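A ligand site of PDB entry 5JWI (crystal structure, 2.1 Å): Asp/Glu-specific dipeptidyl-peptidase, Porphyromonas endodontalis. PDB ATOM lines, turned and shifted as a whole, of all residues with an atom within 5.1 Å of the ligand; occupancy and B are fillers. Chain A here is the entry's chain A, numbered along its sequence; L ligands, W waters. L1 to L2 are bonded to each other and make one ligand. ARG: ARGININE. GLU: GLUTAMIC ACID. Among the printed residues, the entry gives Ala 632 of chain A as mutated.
Trp 198 touches the ligand. OE1 of Gln 311 touches NH2 of ARG L1, at 3.6 Å. CA of Gly 629 touches OXT of GLU L2, 3.3 Å away. N of Asn 631 touches OXT of GLU L2 (3.7 Å). 17 residues have an atom within 4 Å of the ligand: His 65, Ser 193, Asn 197, Trp 198, Ala 308, Gln 311, Asn 312, Thr 627, Thr 628, Gly 629, Gly 630, Asn 631, Ala 632, Asn 647, Phe 648, Asp 649 and Arg 650. The nearest printed residue that does not touch the ligand is Arg 202 (4.1 Å).
The side-chain hydroxyl (OG) of Ser 668 is in hydrogen-bond range of the side-chain hydroxyl (OG1) of Thr 627. The side-chain carboxylate of Asp 649 lies within salt-bridge range of the guanidinium group of Arg 202, at 2.8 Å. The side-chain amide nitrogen of Asn 197 lies within hydrogen-bond range of the side-chain amide oxygen of Asn 312 (3.0 Å). N of Thr 628 is in hydrogen-bond range of OD1 of Asn 631 (3.2 Å). The side-chain amide nitrogen of Gln 311 is in hydrogen-bond range of the backbone carbonyl oxygen of Asp 194 (3.4 Å). The side-chain amide nitrogen of Asn 197 lies within hydrogen-bond range of the side-chain amide oxygen of Gln 311 (3.0 Å). The side-chain carboxylate of Asp 206 sits at hydrogen-bond distance from a ring nitrogen (ND1) of His 65 (2.6 Å). OD1 of Asn 197 sits close to OD2 of Asp 649 (3.3 Å).
Water W3 bridges O of ARG L1 and NH1 of Arg 316.
OE1 of GLU L2 is in hydrogen-bond range of ND2 of Asn 647 (2.8 Å). OG1 of Thr 627 sits at hydrogen-bond distance from OE1 of GLU L2, at 2.9 Å. N of Thr 628 sits close to OE2 of GLU L2, at 3.4 Å. A ring nitrogen (NE2) of His 65 is in hydrogen-bond range of an oxygen (O) of GLU L2, 2.8 Å away. OD1 of Asp 649 lies within salt-bridge range of N of ARG L1, 2.8 Å away. NH1 of ARG L1 sits at hydrogen-bond distance from O of Ser 193 (3.1 Å). The backbone carbonyl oxygen (O) of Ala 308 is in hydrogen-bond range of a nitrogen (NH2) of ARG L1, at 3.0 Å. N of ARG L1 lies within hydrogen-bond range of OD1 of Asn 197, at 2.7 Å. O of Phe 648 lies within hydrogen-bond range of N of GLU L2 (3.0 Å). The backbone NH (N) of Ala 632 sits close to an oxygen (OXT) of GLU L2 (3.2 Å). A nitrogen (N) of ARG L1 sits at hydrogen-bond distance from the side-chain amide oxygen of Asn 312 (2.8 Å). The guanidinium group of Arg 650 is in salt-bridge range of an oxygen (OE2) of GLU L2 (2.9 Å). An oxygen (OXT) of GLU L2 sits at hydrogen-bond distance from the backbone NH (N) of Gly 630.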
ATOM      1  N   GLY A  48     -32.830 -30.764 -31.446  1.00  0.00           N
ATOM      2  CA  GLY A  48     -31.890 -29.940 -30.713  1.00  0.00           C
ATOM      3  C   GLY A  48     -32.397 -28.667 -30.040  1.00  0.00           C
ATOM      4  O   GLY A  48     -31.615 -27.898 -29.509  1.00  0.00           O
ATOM      5  N   HIS A  65     -34.710 -18.874 -34.538  1.00  0.00           N
ATOM      6  CA  HIS A  65     -33.525 -19.574 -35.008  1.00  0.00           C
ATOM      7  C   HIS A  65     -33.705 -21.081 -34.840  1.00  0.00           C
ATOM      8  O   HIS A  65     -32.981 -21.847 -35.471  1.00  0.00           O
ATOM      9  CB  HIS A  65     -32.263 -19.052 -34.298  1.00  0.00           C
ATOM     10  CG  HIS A  65     -32.069 -19.528 -32.895  1.00  0.00           C
ATOM     11  ND1 HIS A  65     -32.430 -18.766 -31.787  1.00  0.00           N
ATOM     12  CD2 HIS A  65     -31.505 -20.653 -32.396  1.00  0.00           C
ATOM     13  CE1 HIS A  65     -32.102 -19.405 -30.681  1.00  0.00           C
ATOM     14  NE2 HIS A  65     -31.531 -20.564 -31.025  1.00  0.00           N
ATOM     15  N   SER A 193     -27.923 -10.073 -35.887  1.00  0.00           N
ATOM     16  CA  SER A 193     -27.651 -11.516 -35.926  1.00  0.00           C
ATOM     17  C   SER A 193     -26.258 -11.912 -35.456  1.00  0.00           C
ATOM     18  O   SER A 193     -26.142 -12.767 -34.601  1.00  0.00           O
ATOM     19  CB  SER A 193     -27.850 -12.083 -37.334  1.00  0.00           C
ATOM     20  OG  SER A 193     -27.022 -11.453 -38.270  1.00  0.00           O
ATOM     21  N   ASP A 194     -25.213 -11.291 -36.009  1.00  0.00           N
ATOM     22  CA  ASP A 194     -23.852 -11.686 -35.666  1.00  0.00           C
ATOM     23  C   ASP A 194     -23.352 -10.928 -34.463  1.00  0.00           C
ATOM     24  O   ASP A 194     -22.905 -11.525 -33.479  1.00  0.00           O
ATOM     25  CB  ASP A 194     -22.905 -11.461 -36.865  1.00  0.00           C
ATOM     26  CG  ASP A 194     -23.109 -12.483 -37.993  1.00  0.00           C
ATOM     27  OD1 ASP A 194     -23.958 -13.394 -37.835  1.00  0.00           O
ATOM     28  OD2 ASP A 194     -22.415 -12.375 -39.044  1.00  0.00           O
ATOM     29  N   ASN A 197     -25.270 -11.565 -31.305  1.00  0.00           N
ATOM     30  CA  ASN A 197     -25.326 -12.974 -30.916  1.00  0.00           C
ATOM     31  C   ASN A 197     -24.502 -13.147 -29.647  1.00  0.00           C
ATOM     32  O   ASN A 197     -23.465 -12.492 -29.514  1.00  0.00           O
ATOM     33  CB  ASN A 197     -24.815 -13.887 -32.045  1.00  0.00           C
ATOM     34  CG  ASN A 197     -25.194 -15.348 -31.809  1.00  0.00           C
ATOM     35  OD1 ASN A 197     -25.960 -15.659 -30.923  1.00  0.00           O
ATOM     36  ND2 ASN A 197     -24.650 -16.238 -32.636  1.00  0.00           N
ATOM     37  N   TRP A 198     -24.957 -14.017 -28.734  1.00  0.00           N
ATOM     38  CA  TRP A 198     -24.331 -14.211 -27.421  1.00  0.00           C
ATOM     39  C   TRP A 198     -24.152 -12.913 -26.641  1.00  0.00           C
ATOM     40  O   TRP A 198     -23.234 -12.793 -25.834  1.00  0.00           O
ATOM     41  CB  TRP A 198     -22.959 -14.888 -27.573  1.00  0.00           C
ATOM     42  CG  TRP A 198     -23.062 -16.234 -28.245  1.00  0.00           C
ATOM     43  CD1 TRP A 198     -22.718 -16.540 -29.511  1.00  0.00           C
ATOM     44  CD2 TRP A 198     -23.548 -17.453 -27.656  1.00  0.00           C
ATOM     45  NE1 TRP A 198     -22.947 -17.872 -29.774  1.00  0.00           N
ATOM     46  CE2 TRP A 198     -23.466 -18.455 -28.641  1.00  0.00           C
ATOM     47  CE3 TRP A 198     -24.058 -17.783 -26.395  1.00  0.00           C
ATOM     48  CZ2 TRP A 198     -23.885 -19.766 -28.423  1.00  0.00           C
ATOM     49  CZ3 TRP A 198     -24.468 -19.097 -26.163  1.00  0.00           C
ATOM     50  CH2 TRP A 198     -24.389 -20.061 -27.172  1.00  0.00           C
ATOM     51  N   ARG A 202     -29.930  -7.106 -25.470  1.00  0.00           N
ATOM     52  CA  ARG A 202     -30.383  -7.813 -26.658  1.00  0.00           C
ATOM     53  C   ARG A 202     -31.758  -7.236 -27.037  1.00  0.00           C
ATOM     54  O   ARG A 202     -32.526  -6.847 -26.160  1.00  0.00           O
ATOM     55  CB  ARG A 202     -30.453  -9.323 -26.387  1.00  0.00           C
ATOM     56  CG  ARG A 202     -30.701 -10.180 -27.627  1.00  0.00           C
ATOM     57  CD  ARG A 202     -29.553 -10.093 -28.637  1.00  0.00           C
ATOM     58  NE  ARG A 202     -29.431 -11.314 -29.434  1.00  0.00           N
ATOM     59  CZ  ARG A 202     -28.855 -12.436 -28.994  1.00  0.00           C
ATOM     60  NH1 ARG A 202     -28.334 -12.477 -27.760  1.00  0.00           N
ATOM     61  NH2 ARG A 202     -28.771 -13.505 -29.781  1.00  0.00           N
ATOM     62  N   ASP A 206     -36.819 -13.157 -31.221  1.00  0.00           N
ATOM     63  CA  ASP A 206     -36.473 -14.513 -31.611  1.00  0.00           C
ATOM     64  C   ASP A 206     -37.625 -15.504 -31.335  1.00  0.00           C
ATOM     65  O   ASP A 206     -37.614 -16.206 -30.311  1.00  0.00           O
ATOM     66  CB  ASP A 206     -35.169 -14.935 -30.880  1.00  0.00           C
ATOM     67  CG  ASP A 206     -34.457 -16.123 -31.547  1.00  0.00           C
ATOM     68  OD1 ASP A 206     -35.034 -16.787 -32.421  1.00  0.00           O
ATOM     69  OD2 ASP A 206     -33.296 -16.403 -31.163  1.00  0.00           O
ATOM     70  N   ALA A 308     -25.583 -19.246 -40.317  1.00  0.00           N
ATOM     71  CA  ALA A 308     -26.026 -18.892 -38.959  1.00  0.00           C
ATOM     72  C   ALA A 308     -25.514 -19.916 -37.934  1.00  0.00           C
ATOM     73  O   ALA A 308     -25.050 -19.561 -36.853  1.00  0.00           O
ATOM     74  CB  ALA A 308     -27.571 -18.792 -38.887  1.00  0.00           C
ATOM     75  N   SER A 309     -25.593 -21.186 -38.294  1.00  0.00           N
ATOM     76  CA  SER A 309     -25.104 -22.259 -37.470  1.00  0.00           C
ATOM     77  C   SER A 309     -23.565 -22.182 -37.294  1.00  0.00           C
ATOM     78  O   SER A 309     -23.053 -22.382 -36.197  1.00  0.00           O
ATOM     79  CB  SER A 309     -25.515 -23.602 -38.067  1.00  0.00           C
ATOM     80  OG  SER A 309     -24.916 -24.675 -37.347  1.00  0.00           O
ATOM     81  N   GLN A 311     -21.557 -19.444 -37.656  1.00  0.00           N
ATOM     82  CA  GLN A 311     -21.263 -18.232 -36.874  1.00  0.00           C
ATOM     83  C   GLN A 311     -21.623 -18.430 -35.395  1.00  0.00           C
ATOM     84  O   GLN A 311     -20.919 -17.941 -34.504  1.00  0.00           O
ATOM     85  CB  GLN A 311     -22.010 -17.027 -37.443  1.00  0.00           C
ATOM     86  CG  GLN A 311     -21.516 -15.671 -36.950  1.00  0.00           C
ATOM     87  CD  GLN A 311     -22.125 -15.271 -35.604  1.00  0.00           C
ATOM     88  OE1 GLN A 311     -23.120 -15.834 -35.171  1.00  0.00           O
ATOM     89  NE2 GLN A 311     -21.504 -14.303 -34.941  1.00  0.00           N
ATOM     90  N   ASN A 312     -22.725 -19.125 -35.139  1.00  0.00           N
ATOM     91  CA  ASN A 312     -23.134 -19.357 -33.755  1.00  0.00           C
ATOM     92  C   ASN A 312     -22.081 -20.148 -32.948  1.00  0.00           C
ATOM     93  O   ASN A 312     -21.731 -19.753 -31.837  1.00  0.00           O
ATOM     94  CB  ASN A 312     -24.476 -20.094 -33.706  1.00  0.00           C
ATOM     95  CG  ASN A 312     -25.051 -20.115 -32.326  1.00  0.00           C
ATOM     96  OD1 ASN A 312     -25.139 -19.080 -31.670  1.00  0.00           O
ATOM     97  ND2 ASN A 312     -25.411 -21.302 -31.851  1.00  0.00           N
ATOM     98  N   ARG A 316     -19.557 -18.726 -30.031  1.00  0.00           N
ATOM     99  CA  ARG A 316     -19.624 -19.428 -28.749  1.00  0.00           C
ATOM    100  C   ARG A 316     -18.211 -19.852 -28.306  1.00  0.00           C
ATOM    101  O   ARG A 316     -17.879 -19.755 -27.127  1.00  0.00           O
ATOM    102  CB  ARG A 316     -20.545 -20.657 -28.817  1.00  0.00           C
ATOM    103  CG  ARG A 316     -20.714 -21.364 -27.445  1.00  0.00           C
ATOM    104  CD  ARG A 316     -21.690 -22.545 -27.522  1.00  0.00           C
ATOM    105  NE  ARG A 316     -21.214 -23.554 -28.451  1.00  0.00           N
ATOM    106  CZ  ARG A 316     -21.862 -23.970 -29.527  1.00  0.00           C
ATOM    107  NH1 ARG A 316     -23.053 -23.496 -29.841  1.00  0.00           N
ATOM    108  NH2 ARG A 316     -21.295 -24.880 -30.297  1.00  0.00           N
ATOM    109  N   THR A 627     -29.008 -21.961 -18.288  1.00  0.00           N
ATOM    110  CA  THR A 627     -29.299 -22.606 -19.579  1.00  0.00           C
ATOM    111  C   THR A 627     -28.071 -22.864 -20.442  1.00  0.00           C
ATOM    112  O   THR A 627     -26.993 -22.288 -20.212  1.00  0.00           O
ATOM    113  CB  THR A 627     -30.257 -21.754 -20.423  1.00  0.00           C
ATOM    114  OG1 THR A 627     -29.735 -20.434 -20.546  1.00  0.00           O
ATOM    115  CG2 THR A 627     -31.671 -21.705 -19.784  1.00  0.00           C
ATOM    116  N   THR A 628     -28.244 -23.702 -21.459  1.00  0.00           N
ATOM    117  CA  THR A 628     -27.214 -23.889 -22.470  1.00  0.00           C
ATOM    118  C   THR A 628     -27.875 -24.261 -23.791  1.00  0.00           C
ATOM    119  O   THR A 628     -29.115 -24.337 -23.873  1.00  0.00           O
ATOM    120  CB  THR A 628     -26.162 -24.986 -22.050  1.00  0.00           C
ATOM    121  OG1 THR A 628     -25.072 -24.997 -22.985  1.00  0.00           O
ATOM    122  CG2 THR A 628     -26.779 -26.390 -21.973  1.00  0.00           C
ATOM    123  N   GLY A 629     -27.045 -24.450 -24.823  1.00  0.00           N
ATOM    124  CA  GLY A 629     -27.518 -24.825 -26.144  1.00  0.00           C
ATOM    125  C   GLY A 629     -28.457 -26.020 -26.037  1.00  0.00           C
ATOM    126  O   GLY A 629     -28.154 -26.994 -25.335  1.00  0.00           O
ATOM    127  N   GLY A 630     -29.597 -25.930 -26.725  1.00  0.00           N
ATOM    128  CA  GLY A 630     -30.684 -26.899 -26.553  1.00  0.00           C
ATOM    129  C   GLY A 630     -31.855 -26.241 -25.810  1.00  0.00           C
ATOM    130  O   GLY A 630     -33.029 -26.597 -26.027  1.00  0.00           O
ATOM    131  N   ASN A 631     -31.555 -25.273 -24.937  1.00  0.00           N
ATOM    132  CA  ASN A 631     -32.588 -24.531 -24.200  1.00  0.00           C
ATOM    133  C   ASN A 631     -33.273 -23.428 -25.018  1.00  0.00           C
ATOM    134  O   ASN A 631     -34.183 -22.777 -24.526  1.00  0.00           O
ATOM    135  CB  ASN A 631     -32.039 -23.877 -22.940  1.00  0.00           C
ATOM    136  CG  ASN A 631     -32.120 -24.775 -21.719  1.00  0.00           C
ATOM    137  OD1 ASN A 631     -31.101 -25.073 -21.087  1.00  0.00           O
ATOM    138  ND2 ASN A 631     -33.326 -25.175 -21.355  1.00  0.00           N
ATOM    139  N   ALA A 632     -32.809 -23.198 -26.241  1.00  0.00           N
ATOM    140  CA  ALA A 632     -33.485 -22.263 -27.131  1.00  0.00           C
ATOM    141  C   ALA A 632     -34.935 -22.690 -27.317  1.00  0.00           C
ATOM    142  O   ALA A 632     -35.214 -23.870 -27.549  1.00  0.00           O
ATOM    143  CB  ALA A 632     -32.790 -22.177 -28.471  1.00  0.00           C
ATOM    144  N   ASN A 647     -36.956 -18.478 -23.735  1.00  0.00           N
ATOM    145  CA  ASN A 647     -35.499 -18.435 -23.730  1.00  0.00           C
ATOM    146  C   ASN A 647     -34.943 -18.478 -25.140  1.00  0.00           C
ATOM    147  O   ASN A 647     -35.470 -19.223 -25.952  1.00  0.00           O
ATOM    148  CB  ASN A 647     -34.912 -19.605 -22.945  1.00  0.00           C
ATOM    149  CG  ASN A 647     -33.399 -19.442 -22.754  1.00  0.00           C
ATOM    150  OD1 ASN A 647     -32.953 -18.518 -22.095  1.00  0.00           O
ATOM    151  ND2 ASN A 647     -32.633 -20.306 -23.379  1.00  0.00           N
ATOM    152  N   PHE A 648     -33.890 -17.721 -25.470  1.00  0.00           N
ATOM    153  CA  PHE A 648     -33.221 -17.970 -26.760  1.00  0.00           C
ATOM    154  C   PHE A 648     -31.703 -17.870 -26.770  1.00  0.00           C
ATOM    155  O   PHE A 648     -31.080 -18.262 -27.741  1.00  0.00           O
ATOM    156  CB  PHE A 648     -33.763 -17.059 -27.881  1.00  0.00           C
ATOM    157  CG  PHE A 648     -33.549 -15.571 -27.687  1.00  0.00           C
ATOM    158  CD1 PHE A 648     -34.410 -14.816 -26.879  1.00  0.00           C
ATOM    159  CD2 PHE A 648     -32.577 -14.894 -28.419  1.00  0.00           C
ATOM    160  CE1 PHE A 648     -34.234 -13.433 -26.738  1.00  0.00           C
ATOM    161  CE2 PHE A 648     -32.405 -13.519 -28.299  1.00  0.00           C
ATOM    162  CZ  PHE A 648     -33.253 -12.783 -27.462  1.00  0.00           C
ATOM    163  N   ASP A 649     -31.110 -17.335 -25.701  1.00  0.00           N
ATOM    164  CA  ASP A 649     -29.642 -17.152 -25.680  1.00  0.00           C
ATOM    165  C   ASP A 649     -29.123 -17.056 -24.252  1.00  0.00           C
ATOM    166  O   ASP A 649     -29.880 -17.136 -23.294  1.00  0.00           O
ATOM    167  CB  ASP A 649     -29.197 -15.904 -26.469  1.00  0.00           C
ATOM    168  CG  ASP A 649     -27.849 -16.095 -27.200  1.00  0.00           C
ATOM    169  OD1 ASP A 649     -27.162 -17.122 -26.935  1.00  0.00           O
ATOM    170  OD2 ASP A 649     -27.454 -15.234 -28.026  1.00  0.00           O
ATOM    171  N   ARG A 650     -27.828 -16.817 -24.158  1.00  0.00           N
ATOM    172  CA  ARG A 650     -27.072 -16.710 -22.925  1.00  0.00           C
ATOM    173  C   ARG A 650     -26.149 -15.526 -23.137  1.00  0.00           C
ATOM    174  O   ARG A 650     -25.715 -15.311 -24.265  1.00  0.00           O
ATOM    175  CB  ARG A 650     -26.293 -18.014 -22.718  1.00  0.00           C
ATOM    176  CG  ARG A 650     -25.401 -18.134 -21.542  1.00  0.00           C
ATOM    177  CD  ARG A 650     -25.201 -19.611 -21.242  1.00  0.00           C
ATOM    178  NE  ARG A 650     -23.969 -20.187 -21.745  1.00  0.00           N
ATOM    179  CZ  ARG A 650     -23.897 -21.046 -22.756  1.00  0.00           C
ATOM    180  NH1 ARG A 650     -25.005 -21.383 -23.417  1.00  0.00           N
ATOM    181  NH2 ARG A 650     -22.732 -21.554 -23.127  1.00  0.00           N
ATOM    182  N   SER A 668     -29.537 -16.045 -18.605  1.00  0.00           N
ATOM    183  CA  SER A 668     -30.316 -16.434 -19.785  1.00  0.00           C
ATOM    184  C   SER A 668     -30.910 -15.185 -20.449  1.00  0.00           C
ATOM    185  O   SER A 668     -31.311 -14.251 -19.759  1.00  0.00           O
ATOM    186  CB  SER A 668     -31.471 -17.384 -19.428  1.00  0.00           C
ATOM    187  OG  SER A 668     -31.023 -18.637 -18.950  1.00  0.00           O
HETATM  188  N   ARG L   1     -26.607 -17.875 -29.620  1.00  0.00           N
HETATM  189  CA  ARG L   1     -27.955 -18.460 -29.655  1.00  0.00           C
HETATM  190  C   ARG L   1     -27.898 -19.863 -29.064  1.00  0.00           C
HETATM  191  O   ARG L   1     -26.991 -20.636 -29.375  1.00  0.00           O
HETATM  192  CB  ARG L   1     -28.519 -18.511 -31.077  1.00  0.00           C
HETATM  193  CG  ARG L   1     -28.938 -17.148 -31.658  1.00  0.00           C
HETATM  194  CD  ARG L   1     -29.348 -17.247 -33.139  1.00  0.00           C
HETATM  195  NE  ARG L   1     -28.231 -17.672 -33.999  1.00  0.00           N
HETATM  196  CZ  ARG L   1     -27.352 -16.839 -34.556  1.00  0.00           C
HETATM  197  NH1 ARG L   1     -27.461 -15.520 -34.357  1.00  0.00           N
HETATM  198  NH2 ARG L   1     -26.349 -17.316 -35.300  1.00  0.00           N
HETATM  199  N   GLU L   2     -28.902 -20.211 -28.251  1.00  0.00           N
HETATM  200  CA  GLU L   2     -28.851 -21.485 -27.579  1.00  0.00           C
HETATM  201  C   GLU L   2     -29.637 -22.522 -28.378  1.00  0.00           C
HETATM  202  O   GLU L   2     -29.849 -22.316 -29.573  1.00  0.00           O
HETATM  203  CB  GLU L   2     -29.339 -21.345 -26.137  1.00  0.00           C
HETATM  204  CG  GLU L   2     -28.223 -20.778 -25.198  1.00  0.00           C
HETATM  205  CD  GLU L   2     -28.643 -20.660 -23.736  1.00  0.00           C
HETATM  206  OE1 GLU L   2     -29.869 -20.586 -23.439  1.00  0.00           O
HETATM  207  OE2 GLU L   2     -27.739 -20.684 -22.874  1.00  0.00           O
HETATM  208  OXT GLU L   2     -30.072 -23.563 -27.884  1.00  0.00           O
HETATM  209  O   HOH W   1     -29.464 -13.926 -33.284  1.00  0.00           O
HETATM  210  O   HOH W   2     -28.019 -20.462 -34.761  1.00  0.00           O
HETATM  211  O   HOH W   3     -25.505 -22.854 -28.551  1.00  0.00           O
